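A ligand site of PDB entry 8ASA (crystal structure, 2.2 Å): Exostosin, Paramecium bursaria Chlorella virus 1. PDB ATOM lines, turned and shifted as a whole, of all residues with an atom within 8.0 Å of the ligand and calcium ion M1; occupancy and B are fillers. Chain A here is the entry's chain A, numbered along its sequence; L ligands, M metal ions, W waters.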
ATOM      1  N   ARG A 165      -6.206   7.470 -23.313  1.00  0.00           N
ATOM      2  CA  ARG A 165      -6.217   8.398 -24.483  1.00  0.00           C
ATOM      3  C   ARG A 165      -4.774   8.765 -24.865  1.00  0.00           C
ATOM      4  O   ARG A 165      -4.450   8.754 -26.086  1.00  0.00           O
ATOM      5  CB  ARG A 165      -7.022   9.663 -24.177  1.00  0.00           C
ATOM      6  CG  ARG A 165      -8.505   9.436 -23.895  1.00  0.00           C
ATOM      7  CD  ARG A 165      -9.318  10.666 -24.257  1.00  0.00           C
ATOM      8  NE  ARG A 165      -9.441  10.771 -25.704  1.00  0.00           N
ATOM      9  CZ  ARG A 165      -9.829  11.851 -26.374  1.00  0.00           C
ATOM     10  NH1 ARG A 165     -10.140  12.965 -25.733  1.00  0.00           N
ATOM     11  NH2 ARG A 165      -9.905  11.818 -27.697  1.00  0.00           N
ATOM     12  N   LEU A 169      -3.534   7.726 -28.425  1.00  0.00           N
ATOM     13  CA  LEU A 169      -3.358   8.806 -29.421  1.00  0.00           C
ATOM     14  C   LEU A 169      -1.886   8.966 -29.843  1.00  0.00           C
ATOM     15  O   LEU A 169      -1.674   9.273 -31.018  1.00  0.00           O
ATOM     16  CB  LEU A 169      -3.906  10.115 -28.846  1.00  0.00           C
ATOM     17  CG  LEU A 169      -5.427  10.203 -28.783  1.00  0.00           C
ATOM     18  CD1 LEU A 169      -5.866  11.392 -27.939  1.00  0.00           C
ATOM     19  CD2 LEU A 169      -6.030  10.284 -30.177  1.00  0.00           C
ATOM     20  N   TYR A 170      -0.907   8.789 -28.943  1.00  0.00           N
ATOM     21  CA  TYR A 170       0.452   9.353 -29.170  1.00  0.00           C
ATOM     22  C   TYR A 170       1.584   8.326 -29.056  1.00  0.00           C
ATOM     23  O   TYR A 170       2.742   8.746 -29.264  1.00  0.00           O
ATOM     24  CB  TYR A 170       0.694  10.528 -28.208  1.00  0.00           C
ATOM     25  CG  TYR A 170      -0.385  11.570 -28.263  1.00  0.00           C
ATOM     26  CD1 TYR A 170      -0.652  12.246 -29.443  1.00  0.00           C
ATOM     27  CD2 TYR A 170      -1.154  11.881 -27.154  1.00  0.00           C
ATOM     28  CE1 TYR A 170      -1.637  13.216 -29.518  1.00  0.00           C
ATOM     29  CE2 TYR A 170      -2.133  12.847 -27.200  1.00  0.00           C
ATOM     30  CZ  TYR A 170      -2.388  13.512 -28.395  1.00  0.00           C
ATOM     31  OH  TYR A 170      -3.362  14.453 -28.473  1.00  0.00           O
ATOM     32  N   PHE A 202       4.671  13.837 -20.574  1.00  0.00           N
ATOM     33  CA  PHE A 202       3.233  13.635 -20.254  1.00  0.00           C
ATOM     34  C   PHE A 202       3.129  13.407 -18.745  1.00  0.00           C
ATOM     35  O   PHE A 202       3.731  12.432 -18.264  1.00  0.00           O
ATOM     36  CB  PHE A 202       2.664  12.436 -21.014  1.00  0.00           C
ATOM     37  CG  PHE A 202       2.368  12.672 -22.470  1.00  0.00           C
ATOM     38  CD1 PHE A 202       1.245  13.394 -22.857  1.00  0.00           C
ATOM     39  CD2 PHE A 202       3.167  12.131 -23.465  1.00  0.00           C
ATOM     40  CE1 PHE A 202       0.946  13.578 -24.198  1.00  0.00           C
ATOM     41  CE2 PHE A 202       2.878  12.329 -24.803  1.00  0.00           C
ATOM     42  CZ  PHE A 202       1.763  13.063 -25.172  1.00  0.00           C
ATOM     43  N   ILE A 225       3.146  18.147 -19.127  1.00  0.00           N
ATOM     44  CA  ILE A 225       1.816  18.399 -19.729  1.00  0.00           C
ATOM     45  C   ILE A 225       0.774  17.792 -18.807  1.00  0.00           C
ATOM     46  O   ILE A 225       0.889  16.584 -18.520  1.00  0.00           O
ATOM     47  CB  ILE A 225       1.722  17.852 -21.157  1.00  0.00           C
ATOM     48  CG1 ILE A 225       2.929  18.269 -22.000  1.00  0.00           C
ATOM     49  CG2 ILE A 225       0.406  18.255 -21.808  1.00  0.00           C
ATOM     50  CD1 ILE A 225       3.121  17.465 -23.258  1.00  0.00           C
ATOM     51  N   VAL A 226      -0.184  18.603 -18.355  1.00  0.00           N
ATOM     52  CA  VAL A 226      -1.178  18.271 -17.294  1.00  0.00           C
ATOM     53  C   VAL A 226      -2.549  18.829 -17.691  1.00  0.00           C
ATOM     54  O   VAL A 226      -2.606  19.969 -18.196  1.00  0.00           O
ATOM     55  CB  VAL A 226      -0.743  18.839 -15.935  1.00  0.00           C
ATOM     56  CG1 VAL A 226      -1.691  18.452 -14.826  1.00  0.00           C
ATOM     57  CG2 VAL A 226       0.693  18.448 -15.592  1.00  0.00           C
ATOM     58  N   LYS A 227      -3.627  18.083 -17.427  1.00  0.00           N
ATOM     59  CA  LYS A 227      -5.023  18.515 -17.695  1.00  0.00           C
ATOM     60  C   LYS A 227      -5.436  19.530 -16.628  1.00  0.00           C
ATOM     61  O   LYS A 227      -5.188  19.257 -15.428  1.00  0.00           O
ATOM     62  CB  LYS A 227      -5.980  17.324 -17.695  1.00  0.00           C
ATOM     63  CG  LYS A 227      -7.384  17.624 -18.192  1.00  0.00           C
ATOM     64  CD  LYS A 227      -8.199  16.391 -18.519  1.00  0.00           C
ATOM     65  CE  LYS A 227      -9.523  16.701 -19.177  1.00  0.00           C
ATOM     66  NZ  LYS A 227     -10.562  17.054 -18.174  1.00  0.00           N
ATOM     67  N   LYS A 228      -6.036  20.642 -17.060  1.00  0.00           N
ATOM     68  CA  LYS A 228      -6.549  21.721 -16.169  1.00  0.00           C
ATOM     69  C   LYS A 228      -7.421  21.095 -15.071  1.00  0.00           C
ATOM     70  O   LYS A 228      -8.226  20.200 -15.363  1.00  0.00           O
ATOM     71  CB  LYS A 228      -7.354  22.754 -16.961  1.00  0.00           C
ATOM     72  CG  LYS A 228      -6.521  23.644 -17.861  1.00  0.00           C
ATOM     73  CD  LYS A 228      -7.329  24.536 -18.775  1.00  0.00           C
ATOM     74  CE  LYS A 228      -6.466  25.405 -19.667  1.00  0.00           C
ATOM     75  NZ  LYS A 228      -7.276  26.175 -20.627  1.00  0.00           N
ATOM     76  N   LEU A 241       2.498  22.940 -18.870  1.00  0.00           N
ATOM     77  CA  LEU A 241       1.584  23.057 -20.045  1.00  0.00           C
ATOM     78  C   LEU A 241       0.222  22.481 -19.633  1.00  0.00           C
ATOM     79  O   LEU A 241       0.101  21.235 -19.539  1.00  0.00           O
ATOM     80  CB  LEU A 241       2.164  22.356 -21.276  1.00  0.00           C
ATOM     81  CG  LEU A 241       1.301  22.437 -22.529  1.00  0.00           C
ATOM     82  CD1 LEU A 241       0.749  23.833 -22.742  1.00  0.00           C
ATOM     83  CD2 LEU A 241       2.077  21.977 -23.752  1.00  0.00           C
ATOM     84  N   PHE A 242      -0.742  23.370 -19.379  1.00  0.00           N
ATOM     85  CA  PHE A 242      -2.118  23.007 -18.966  1.00  0.00           C
ATOM     86  C   PHE A 242      -2.978  22.858 -20.209  1.00  0.00           C
ATOM     87  O   PHE A 242      -2.988  23.762 -21.059  1.00  0.00           O
ATOM     88  CB  PHE A 242      -2.673  24.029 -17.974  1.00  0.00           C
ATOM     89  CG  PHE A 242      -2.036  23.968 -16.616  1.00  0.00           C
ATOM     90  CD1 PHE A 242      -2.111  22.817 -15.855  1.00  0.00           C
ATOM     91  CD2 PHE A 242      -1.343  25.049 -16.102  1.00  0.00           C
ATOM     92  CE1 PHE A 242      -1.520  22.742 -14.606  1.00  0.00           C
ATOM     93  CE2 PHE A 242      -0.752  24.988 -14.851  1.00  0.00           C
ATOM     94  CZ  PHE A 242      -0.835  23.824 -14.108  1.00  0.00           C
ATOM     95  N   VAL A 243      -3.671  21.720 -20.314  1.00  0.00           N
ATOM     96  CA  VAL A 243      -4.484  21.358 -21.502  1.00  0.00           C
ATOM     97  C   VAL A 243      -5.947  21.254 -21.070  1.00  0.00           C
ATOM     98  O   VAL A 243      -6.210  20.930 -19.890  1.00  0.00           O
ATOM     99  CB  VAL A 243      -3.928  20.073 -22.143  1.00  0.00           C
ATOM    100  CG1 VAL A 243      -2.493  20.250 -22.597  1.00  0.00           C
ATOM    101  CG2 VAL A 243      -4.043  18.861 -21.216  1.00  0.00           C
ATOM    102  N   ASN A 244      -6.878  21.598 -21.977  1.00  0.00           N
ATOM    103  CA  ASN A 244      -8.342  21.462 -21.773  1.00  0.00           C
ATOM    104  C   ASN A 244      -8.698  19.969 -21.866  1.00  0.00           C
ATOM    105  O   ASN A 244      -9.599  19.536 -21.132  1.00  0.00           O
ATOM    106  CB  ASN A 244      -9.137  22.290 -22.788  1.00  0.00           C
ATOM    107  CG  ASN A 244      -8.956  23.782 -22.580  1.00  0.00           C
ATOM    108  OD1 ASN A 244      -8.945  24.253 -21.446  1.00  0.00           O
ATOM    109  ND2 ASN A 244      -8.813  24.524 -23.665  1.00  0.00           N
ATOM    110  N   ASP A 245      -7.994  19.227 -22.721  1.00  0.00           N
ATOM    111  CA  ASP A 245      -8.205  17.777 -22.926  1.00  0.00           C
ATOM    112  C   ASP A 245      -6.914  17.187 -23.500  1.00  0.00           C
ATOM    113  O   ASP A 245      -5.936  17.936 -23.604  1.00  0.00           O
ATOM    114  CB  ASP A 245      -9.442  17.542 -23.803  1.00  0.00           C
ATOM    115  CG  ASP A 245      -9.312  18.017 -25.230  1.00  0.00           C
ATOM    116  OD1 ASP A 245      -8.165  18.189 -25.719  1.00  0.00           O
ATOM    117  OD2 ASP A 245     -10.363  18.192 -25.873  1.00  0.00           O
ATOM    118  N   TRP A 246      -6.935  15.918 -23.880  1.00  0.00           N
ATOM    119  CA  TRP A 246      -5.728  15.179 -24.327  1.00  0.00           C
ATOM    120  C   TRP A 246      -5.716  15.006 -25.847  1.00  0.00           C
ATOM    121  O   TRP A 246      -4.722  14.457 -26.380  1.00  0.00           O
ATOM    122  CB  TRP A 246      -5.660  13.860 -23.558  1.00  0.00           C
ATOM    123  CG  TRP A 246      -5.257  14.090 -22.137  1.00  0.00           C
ATOM    124  CD1 TRP A 246      -6.021  13.986 -21.015  1.00  0.00           C
ATOM    125  CD2 TRP A 246      -3.957  14.533 -21.713  1.00  0.00           C
ATOM    126  NE1 TRP A 246      -5.267  14.301 -19.913  1.00  0.00           N
ATOM    127  CE2 TRP A 246      -4.004  14.649 -20.306  1.00  0.00           C
ATOM    128  CE3 TRP A 246      -2.770  14.831 -22.380  1.00  0.00           C
ATOM    129  CZ2 TRP A 246      -2.905  15.048 -19.559  1.00  0.00           C
ATOM    130  CZ3 TRP A 246      -1.679  15.232 -21.649  1.00  0.00           C
ATOM    131  CH2 TRP A 246      -1.744  15.328 -20.254  1.00  0.00           C
ATOM    132  N   GLU A 247      -6.718  15.545 -26.533  1.00  0.00           N
ATOM    133  CA  GLU A 247      -6.914  15.343 -27.997  1.00  0.00           C
ATOM    134  C   GLU A 247      -6.290  16.482 -28.786  1.00  0.00           C
ATOM    135  O   GLU A 247      -6.425  17.652 -28.353  1.00  0.00           O
ATOM    136  CB  GLU A 247      -8.409  15.267 -28.285  1.00  0.00           C
ATOM    137  CG  GLU A 247      -8.708  14.810 -29.697  1.00  0.00           C
ATOM    138  CD  GLU A 247     -10.193  14.705 -29.973  1.00  0.00           C
ATOM    139  OE1 GLU A 247     -10.946  14.486 -29.003  1.00  0.00           O
ATOM    140  OE2 GLU A 247     -10.582  14.841 -31.153  1.00  0.00           O
ATOM    141  N   ASN A 248      -5.668  16.169 -29.927  1.00  0.00           N
ATOM    142  CA  ASN A 248      -5.205  17.149 -30.946  1.00  0.00           C
ATOM    143  C   ASN A 248      -3.893  17.816 -30.487  1.00  0.00           C
ATOM    144  O   ASN A 248      -3.639  18.976 -30.901  1.00  0.00           O
ATOM    145  CB  ASN A 248      -6.282  18.184 -31.260  1.00  0.00           C
ATOM    146  CG  ASN A 248      -7.488  17.556 -31.923  1.00  0.00           C
ATOM    147  OD1 ASN A 248      -8.621  17.812 -31.529  1.00  0.00           O
ATOM    148  ND2 ASN A 248      -7.250  16.716 -32.907  1.00  0.00           N
ATOM    149  N   ILE A 249      -3.084  17.126 -29.688  1.00  0.00           N
ATOM    150  CA  ILE A 249      -1.666  17.516 -29.473  1.00  0.00           C
ATOM    151  C   ILE A 249      -0.925  17.186 -30.760  1.00  0.00           C
ATOM    152  O   ILE A 249      -1.018  16.033 -31.225  1.00  0.00           O
ATOM    153  CB  ILE A 249      -1.041  16.831 -28.249  1.00  0.00           C
ATOM    154  CG1 ILE A 249      -1.734  17.271 -26.962  1.00  0.00           C
ATOM    155  CG2 ILE A 249       0.462  17.101 -28.220  1.00  0.00           C
ATOM    156  CD1 ILE A 249      -1.292  16.521 -25.727  1.00  0.00           C
ATOM    157  N   THR A 250      -0.235  18.168 -31.333  1.00  0.00           N
ATOM    158  CA  THR A 250       0.577  18.025 -32.564  1.00  0.00           C
ATOM    159  C   THR A 250       1.993  18.525 -32.268  1.00  0.00           C
ATOM    160  O   THR A 250       2.190  19.161 -31.195  1.00  0.00           O
ATOM    161  CB  THR A 250      -0.045  18.796 -33.739  1.00  0.00           C
ATOM    162  OG1 THR A 250       0.095  20.187 -33.435  1.00  0.00           O
ATOM    163  CG2 THR A 250      -1.492  18.449 -33.966  1.00  0.00           C
ATOM    164  N   TYR A 253       1.717  22.387 -32.366  1.00  0.00           N
ATOM    165  CA  TYR A 253       1.155  22.889 -31.082  1.00  0.00           C
ATOM    166  C   TYR A 253       2.238  22.881 -29.993  1.00  0.00           C
ATOM    167  O   TYR A 253       2.433  23.936 -29.364  1.00  0.00           O
ATOM    168  CB  TYR A 253      -0.085  22.093 -30.650  1.00  0.00           C
ATOM    169  CG  TYR A 253      -0.451  22.322 -29.209  1.00  0.00           C
ATOM    170  CD1 TYR A 253      -1.213  23.414 -28.828  1.00  0.00           C
ATOM    171  CD2 TYR A 253       0.005  21.472 -28.224  1.00  0.00           C
ATOM    172  CE1 TYR A 253      -1.525  23.646 -27.495  1.00  0.00           C
ATOM    173  CE2 TYR A 253      -0.287  21.690 -26.890  1.00  0.00           C
ATOM    174  CZ  TYR A 253      -1.067  22.770 -26.528  1.00  0.00           C
ATOM    175  OH  TYR A 253      -1.366  22.976 -25.211  1.00  0.00           O
ATOM    176  N   LEU A 254       2.938  21.764 -29.794  1.00  0.00           N
ATOM    177  CA  LEU A 254       3.988  21.632 -28.741  1.00  0.00           C
ATOM    178  C   LEU A 254       5.175  22.561 -29.016  1.00  0.00           C
ATOM    179  O   LEU A 254       5.719  23.101 -28.037  1.00  0.00           O
ATOM    180  CB  LEU A 254       4.466  20.172 -28.655  1.00  0.00           C
ATOM    181  CG  LEU A 254       3.469  19.188 -28.048  1.00  0.00           C
ATOM    182  CD1 LEU A 254       4.035  17.787 -28.108  1.00  0.00           C
ATOM    183  CD2 LEU A 254       3.122  19.562 -26.612  1.00  0.00           C
ATOM    184  N   GLN A 257       4.208  26.010 -27.963  1.00  0.00           N
ATOM    185  CA  GLN A 257       4.081  26.091 -26.477  1.00  0.00           C
ATOM    186  C   GLN A 257       5.497  26.084 -25.872  1.00  0.00           C
ATOM    187  O   GLN A 257       5.717  26.836 -24.910  1.00  0.00           O
ATOM    188  CB  GLN A 257       3.188  24.965 -25.950  1.00  0.00           C
ATOM    189  CG  GLN A 257       1.722  25.134 -26.343  1.00  0.00           C
ATOM    190  CD  GLN A 257       1.111  26.419 -25.823  1.00  0.00           C
ATOM    191  OE1 GLN A 257       1.463  26.903 -24.753  1.00  0.00           O
ATOM    192  NE2 GLN A 257       0.189  26.979 -26.590  1.00  0.00           N
HETATM  193  N1  LIG L   1      -4.868  21.181 -27.504  1.00  0.00           N
HETATM  194  C1  LIG L   1      -4.986  22.295 -26.559  1.00  0.00           C
HETATM  195  C2  LIG L   1      -5.905  22.021 -25.380  1.00  0.00           C
HETATM  196  O1  LIG L   1      -5.722  22.698 -24.354  1.00  0.00           O
HETATM  197  O2  LIG L   1      -6.759  21.124 -25.513  1.00  0.00           O
HETATM  198  C3  LIG L   1      -3.812  20.228 -27.115  1.00  0.00           C
HETATM  199  C4  LIG L   1      -4.083  19.502 -25.821  1.00  0.00           C
HETATM  200  O3  LIG L   1      -5.189  18.633 -25.959  1.00  0.00           O
HETATM  201  C5  LIG L   1      -4.711  21.639 -28.901  1.00  0.00           C
HETATM  202  C6  LIG L   1      -6.000  22.097 -29.540  1.00  0.00           C
HETATM  203  O4  LIG L   1      -6.925  21.023 -29.650  1.00  0.00           O
HETATM  204 CA    CA M   1      -7.030  19.497 -27.234  1.00  0.00          CA
HETATM  205 CA    CA M   2      -8.702  23.919 -26.725  1.00  0.00          CA
HETATM  206 MG    MG M   3      -9.347  14.122 -22.563  1.00  0.00          MG
HETATM  207  O   HOH W   1      -9.094  18.778 -28.123  1.00  0.00           O
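O of Asp 245 sits close to O3 of the ligand, 2.6 Å away. N of Asn 244 is in hydrogen-bond range of O1 of the ligand (2.9 Å). The backbone NH of Glu 247 lies close to an oxygen (O3) of the ligand (3.5 Å).
NZ of Lys 228 sits at hydrogen-bond distance from OD1 of Asn 244 (2.7 Å). The backbone NH of Ile 249 is in hydrogen-bond range of the side-chain hydroxyl of Tyr 170 (2.9 Å). N of Tyr 253 is in hydrogen-bond range of OG1 of Thr 250 (2.9 Å). The backbone NH of Asn 248 is in hydrogen-bond range of the side-chain hydroxyl of Tyr 170 (3.2 Å). The backbone carbonyl oxygen (O) of Trp 246 sits at hydrogen-bond distance from the side-chain hydroxyl (OH) of Tyr 170 (2.5 Å). The side-chain carboxylate (OE1) of Glu 247 is in salt-bridge range of the guanidinium group (NH2) of Arg 165 (3.1 Å). N of Val 243 sits at hydrogen-bond distance from O of Val 226 (2.9 Å). N of Lys 228 is in hydrogen-bond range of O of Val 243, 2.8 Å away.
Merely in contact with the ligand: Val 243, Trp 246, Asn 248, Ile 249 and Tyr 253. Within 4 Å of the ligand: Val 243, Asn 244, Asp 245, Trp 246, Glu 247, Asn 248, Ile 249 and Tyr 253. The nearest printed residue that does not touch the ligand is Phe 242 (4.4 Å).
The nearest printed residue that does not touch calcium ion M1 is Asn 248 (4.3 Å).
Calcium ion M1 is bound by O of Glu 247 (2.2 Å), OD1 of Asp 245 (2.3 Å), water W1 (2.4 Å), O2 of the ligand (2.4 Å), O3 of the ligand (2.4 Å), N1 of the ligand (2.8 Å) and O4 of the ligand (2.9 Å). Calcium ion M1 has seven donor atoms within binding distance.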
